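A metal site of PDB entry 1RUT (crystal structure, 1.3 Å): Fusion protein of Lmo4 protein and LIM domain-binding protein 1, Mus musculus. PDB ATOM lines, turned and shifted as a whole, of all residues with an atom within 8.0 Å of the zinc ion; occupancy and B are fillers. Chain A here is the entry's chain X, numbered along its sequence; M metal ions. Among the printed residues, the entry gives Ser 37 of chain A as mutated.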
ATOM      1  N   LYS A  34      23.179   8.815  20.406  1.00  0.00           N
ATOM      2  CA  LYS A  34      21.870   8.192  20.376  1.00  0.00           C
ATOM      3  C   LYS A  34      21.694   7.401  19.097  1.00  0.00           C
ATOM      4  O   LYS A  34      22.268   7.730  18.060  1.00  0.00           O
ATOM      5  CB  LYS A  34      20.757   9.252  20.435  1.00  0.00           C
ATOM      6  CG  LYS A  34      20.694  10.050  21.723  1.00  0.00           C
ATOM      7  CD  LYS A  34      19.757  11.242  21.553  1.00  0.00           C
ATOM      8  CE  LYS A  34      20.398  12.368  20.750  1.00  0.00           C
ATOM      9  NZ  LYS A  34      19.437  13.476  20.503  1.00  0.00           N
ATOM     10  N   CYS A  35      20.907   6.343  19.183  1.00  0.00           N
ATOM     11  CA  CYS A  35      20.547   5.592  17.998  1.00  0.00           C
ATOM     12  C   CYS A  35      19.742   6.447  17.041  1.00  0.00           C
ATOM     13  O   CYS A  35      18.738   7.056  17.418  1.00  0.00           O
ATOM     14  CB  CYS A  35      19.709   4.388  18.382  1.00  0.00           C
ATOM     15  SG  CYS A  35      19.233   3.360  16.966  1.00  0.00           S
ATOM     16  N   SER A  36      20.131   6.453  15.773  1.00  0.00           N
ATOM     17  CA  SER A  36      19.431   7.211  14.752  1.00  0.00           C
ATOM     18  C   SER A  36      17.968   6.790  14.641  1.00  0.00           C
ATOM     19  O   SER A  36      17.095   7.613  14.330  1.00  0.00           O
ATOM     20  CB  SER A  36      20.113   6.990  13.403  1.00  0.00           C
ATOM     21  OG  SER A  36      21.424   7.509  13.382  1.00  0.00           O
ATOM     22  N   SER A  37      17.696   5.501  14.809  1.00  0.00           N
ATOM     23  CA  SER A  37      16.364   4.954  14.649  1.00  0.00           C
ATOM     24  C   SER A  37      15.483   5.105  15.897  1.00  0.00           C
ATOM     25  O   SER A  37      14.350   5.604  15.791  1.00  0.00           O
ATOM     26  CB  SER A  37      16.445   3.495  14.254  1.00  0.00           C
ATOM     27  OG  SER A  37      15.169   2.909  14.137  1.00  0.00           O
ATOM     28  N   CYS A  38      15.944   4.661  17.048  1.00  0.00           N
ATOM     29  CA  CYS A  38      15.101   4.585  18.247  1.00  0.00           C
ATOM     30  C   CYS A  38      15.439   5.609  19.340  1.00  0.00           C
ATOM     31  O   CYS A  38      14.749   5.668  20.353  1.00  0.00           O
ATOM     32  CB  CYS A  38      15.109   3.172  18.830  1.00  0.00           C
ATOM     33  SG  CYS A  38      16.663   2.805  19.719  1.00  0.00           S
ATOM     34  N   GLN A  39      16.515   6.370  19.149  1.00  0.00           N
ATOM     35  CA  GLN A  39      16.956   7.412  20.081  1.00  0.00           C
ATOM     36  C   GLN A  39      17.494   6.897  21.412  1.00  0.00           C
ATOM     37  O   GLN A  39      17.739   7.669  22.310  1.00  0.00           O
ATOM     38  CB  GLN A  39      15.877   8.494  20.316  1.00  0.00           C
ATOM     39  CG  GLN A  39      15.573   9.340  19.115  1.00  0.00           C
ATOM     40  CD  GLN A  39      14.801   8.587  18.073  1.00  0.00           C
ATOM     41  OE1 GLN A  39      13.729   8.033  18.358  1.00  0.00           O
ATOM     42  NE2 GLN A  39      15.341   8.534  16.867  1.00  0.00           N
ATOM     43  N   ALA A  40      17.748   5.596  21.497  1.00  0.00           N
ATOM     44  CA  ALA A  40      18.325   5.042  22.715  1.00  0.00           C
ATOM     45  C   ALA A  40      19.672   5.692  22.991  1.00  0.00           C
ATOM     46  O   ALA A  40      20.429   5.993  22.064  1.00  0.00           O
ATOM     47  CB  ALA A  40      18.516   3.544  22.595  1.00  0.00           C
ATOM     48  N   GLN A  41      19.980   5.874  24.268  1.00  0.00           N
ATOM     49  CA  GLN A  41      21.253   6.415  24.691  1.00  0.00           C
ATOM     50  C   GLN A  41      22.267   5.260  24.720  1.00  0.00           C
ATOM     51  O   GLN A  41      22.314   4.459  25.657  1.00  0.00           O
ATOM     52  CB  GLN A  41      21.140   7.096  26.049  1.00  0.00           C
ATOM     53  CG  GLN A  41      20.315   8.346  25.981  1.00  0.00           C
ATOM     54  CD  GLN A  41      20.291   9.109  27.279  1.00  0.00           C
ATOM     55  OE1 GLN A  41      20.566   8.541  28.337  1.00  0.00           O
ATOM     56  NE2 GLN A  41      19.964  10.398  27.213  1.00  0.00           N
ATOM     57  N   LEU A  42      23.045   5.167  23.653  1.00  0.00           N
ATOM     58  CA  LEU A  42      23.879   4.023  23.336  1.00  0.00           C
ATOM     59  C   LEU A  42      24.862   3.674  24.442  1.00  0.00           C
ATOM     60  O   LEU A  42      25.131   2.494  24.666  1.00  0.00           O
ATOM     61  CB  LEU A  42      24.618   4.261  22.017  1.00  0.00           C
ATOM     62  CG  LEU A  42      23.677   4.391  20.819  1.00  0.00           C
ATOM     63  CD1 LEU A  42      24.448   4.682  19.549  1.00  0.00           C
ATOM     64  CD2 LEU A  42      22.810   3.168  20.645  1.00  0.00           C
ATOM     65  N   ILE A  45      22.718   1.800  27.169  1.00  0.00           N
ATOM     66  CA  ILE A  45      21.987   0.589  26.885  1.00  0.00           C
ATOM     67  C   ILE A  45      22.890  -0.599  26.606  1.00  0.00           C
ATOM     68  O   ILE A  45      22.492  -1.717  26.869  1.00  0.00           O
ATOM     69  CB  ILE A  45      20.936   0.768  25.774  1.00  0.00           C
ATOM     70  CG1 ILE A  45      21.570   1.115  24.416  1.00  0.00           C
ATOM     71  CG2 ILE A  45      19.900   1.819  26.203  1.00  0.00           C
ATOM     72  CD1 ILE A  45      20.743   0.646  23.262  1.00  0.00           C
ATOM     73  N   ILE A  56      24.039   5.926  13.047  1.00  0.00           N
ATOM     74  CA  ILE A  56      24.683   5.358  14.222  1.00  0.00           C
ATOM     75  C   ILE A  56      23.572   4.621  14.949  1.00  0.00           C
ATOM     76  O   ILE A  56      22.588   5.238  15.347  1.00  0.00           O
ATOM     77  CB  ILE A  56      25.306   6.441  15.113  1.00  0.00           C
ATOM     78  CG1 ILE A  56      26.419   7.201  14.386  1.00  0.00           C
ATOM     79  CG2 ILE A  56      25.863   5.808  16.369  1.00  0.00           C
ATOM     80  CD1 ILE A  56      26.935   8.432  15.122  1.00  0.00           C
ATOM     81  N   LEU A  57      23.695   3.306  15.089  1.00  0.00           N
ATOM     82  CA  LEU A  57      22.602   2.456  15.513  1.00  0.00           C
ATOM     83  C   LEU A  57      22.935   1.644  16.750  1.00  0.00           C
ATOM     84  O   LEU A  57      24.069   1.233  16.976  1.00  0.00           O
ATOM     85  CB  LEU A  57      22.219   1.483  14.394  1.00  0.00           C
ATOM     86  CG  LEU A  57      21.700   2.158  13.121  1.00  0.00           C
ATOM     87  CD1 LEU A  57      21.621   1.121  11.997  1.00  0.00           C
ATOM     88  CD2 LEU A  57      20.376   2.826  13.315  1.00  0.00           C
ATOM     89  N   CYS A  58      21.899   1.392  17.549  1.00  0.00           N
ATOM     90  CA  CYS A  58      21.994   0.351  18.569  1.00  0.00           C
ATOM     91  C   CYS A  58      22.044  -1.016  17.891  1.00  0.00           C
ATOM     92  O   CYS A  58      21.685  -1.161  16.722  1.00  0.00           O
ATOM     93  CB  CYS A  58      20.803   0.406  19.531  1.00  0.00           C
ATOM     94  SG  CYS A  58      19.186  -0.084  18.866  1.00  0.00           S
ATOM     95  N   ARG A  59      22.472  -2.019  18.644  1.00  0.00           N
ATOM     96  CA  ARG A  59      22.561  -3.351  18.076  1.00  0.00           C
ATOM     97  C   ARG A  59      21.211  -3.835  17.529  1.00  0.00           C
ATOM     98  O   ARG A  59      21.150  -4.380  16.424  1.00  0.00           O
ATOM     99  CB  ARG A  59      23.077  -4.347  19.102  1.00  0.00           C
ATOM    100  CG  ARG A  59      23.269  -5.753  18.524  1.00  0.00           C
ATOM    101  CD  ARG A  59      23.995  -6.720  19.445  1.00  0.00           C
ATOM    102  NE  ARG A  59      25.400  -6.344  19.584  1.00  0.00           N
ATOM    103  CZ  ARG A  59      26.114  -6.473  20.695  1.00  0.00           C
ATOM    104  NH1 ARG A  59      25.586  -6.961  21.821  1.00  0.00           N
ATOM    105  NH2 ARG A  59      27.385  -6.099  20.694  1.00  0.00           N
ATOM    106  N   ASN A  60      20.139  -3.620  18.276  1.00  0.00           N
ATOM    107  CA  ASN A  60      18.822  -4.100  17.837  1.00  0.00           C
ATOM    108  C   ASN A  60      18.372  -3.484  16.514  1.00  0.00           C
ATOM    109  O   ASN A  60      17.854  -4.170  15.660  1.00  0.00           O
ATOM    110  CB  ASN A  60      17.771  -3.904  18.924  1.00  0.00           C
ATOM    111  CG  ASN A  60      17.943  -4.858  20.094  1.00  0.00           C
ATOM    112  OD1 ASN A  60      17.503  -4.571  21.206  1.00  0.00           O
ATOM    113  ND2 ASN A  60      18.589  -5.988  19.846  1.00  0.00           N
ATOM    114  N   ASP A  61      18.596  -2.179  16.331  1.00  0.00           N
ATOM    115  CA  ASP A  61      18.203  -1.552  15.083  1.00  0.00           C
ATOM    116  C   ASP A  61      19.171  -1.878  13.947  1.00  0.00           C
ATOM    117  O   ASP A  61      18.754  -1.943  12.810  1.00  0.00           O
ATOM    118  CB  ASP A  61      17.991  -0.047  15.271  1.00  0.00           C
ATOM    119  CG  ASP A  61      16.676   0.254  15.940  1.00  0.00           C
ATOM    120  OD1 ASP A  61      15.640  -0.268  15.449  1.00  0.00           O
ATOM    121  OD2 ASP A  61      16.590   1.014  16.945  1.00  0.00           O
ATOM    122  N   TYR A  62      20.442  -2.127  14.260  1.00  0.00           N
ATOM    123  CA  TYR A  62      21.371  -2.610  13.248  1.00  0.00           C
ATOM    124  C   TYR A  62      20.903  -3.958  12.713  1.00  0.00           C
ATOM    125  O   TYR A  62      20.834  -4.177  11.508  1.00  0.00           O
ATOM    126  CB  TYR A  62      22.778  -2.739  13.831  1.00  0.00           C
ATOM    127  CG  TYR A  62      23.794  -3.249  12.843  1.00  0.00           C
ATOM    128  CD1 TYR A  62      24.282  -2.435  11.839  1.00  0.00           C
ATOM    129  CD2 TYR A  62      24.286  -4.540  12.941  1.00  0.00           C
ATOM    130  CE1 TYR A  62      25.229  -2.895  10.937  1.00  0.00           C
ATOM    131  CE2 TYR A  62      25.240  -5.009  12.065  1.00  0.00           C
ATOM    132  CZ  TYR A  62      25.720  -4.180  11.067  1.00  0.00           C
ATOM    133  OH  TYR A  62      26.688  -4.650  10.211  1.00  0.00           O
ATOM    134  N   ARG A  64      17.844  -5.167  12.892  1.00  0.00           N
ATOM    135  CA  ARG A  64      16.552  -4.980  12.242  1.00  0.00           C
ATOM    136  C   ARG A  64      16.712  -4.418  10.825  1.00  0.00           C
ATOM    137  O   ARG A  64      16.049  -4.895   9.885  1.00  0.00           O
ATOM    138  CB  ARG A  64      15.657  -4.085  13.082  1.00  0.00           C
ATOM    139  CG  ARG A  64      14.233  -3.923  12.544  1.00  0.00           C
ATOM    140  CD  ARG A  64      13.365  -3.034  13.400  1.00  0.00           C
ATOM    141  NE  ARG A  64      13.893  -1.674  13.444  1.00  0.00           N
ATOM    142  CZ  ARG A  64      13.680  -0.727  12.548  1.00  0.00           C
ATOM    143  NH1 ARG A  64      12.900  -0.951  11.475  1.00  0.00           N
ATOM    144  NH2 ARG A  64      14.226   0.472  12.700  1.00  0.00           N
ATOM    145  N   LEU A  65      17.571  -3.424  10.655  1.00  0.00           N
ATOM    146  CA  LEU A  65      17.707  -2.765   9.370  1.00  0.00           C
ATOM    147  C   LEU A  65      18.659  -3.468   8.414  1.00  0.00           C
ATOM    148  O   LEU A  65      18.494  -3.335   7.197  1.00  0.00           O
ATOM    149  CB  LEU A  65      18.151  -1.308   9.580  1.00  0.00           C
ATOM    150  CG  LEU A  65      17.121  -0.397  10.257  1.00  0.00           C
ATOM    151  CD1 LEU A  65      17.728   0.922  10.652  1.00  0.00           C
ATOM    152  CD2 LEU A  65      15.907  -0.169   9.352  1.00  0.00           C
HETATM  153 ZN    ZN M   1      17.992   1.764  18.175  1.00  0.00          ZN
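OD2 of Asp 61 binds the zinc ion, at 2.0 Å. The zinc ion is bound by the side-chain sulfur (SG) of Cys 38. The side-chain sulfur (SG) of Cys 58 binds the zinc ion (2.3 Å). The side-chain sulfur (SG) of Cys 35 is bound to the zinc ion, 2.4 Å away. The zinc ion has four donor atoms within binding distance.
Of the 19 residues printed, 4 come within 4 Å of the zinc ion. Along chain A the residues within 4 Å of the zinc ion span positions 35 to 61.
OD1 of Asp 61 lies within hydrogen-bond range of OG of Ser 37 (3.5 Å). NE of Arg 64 lies within salt-bridge range of OD1 of Asp 61. The side-chain sulfur of Cys 38 sits close to the backbone NH of Ala 40. SG of Cys 58 lies close to N of Asn 60 (3.7 Å). The side-chain sulfur of Cys 35 lies close to the backbone NH of Ser 37 (3.4 Å). The backbone NH of Cys 35 is in hydrogen-bond range of the backbone carbonyl oxygen of Ala 40 (2.9 Å).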
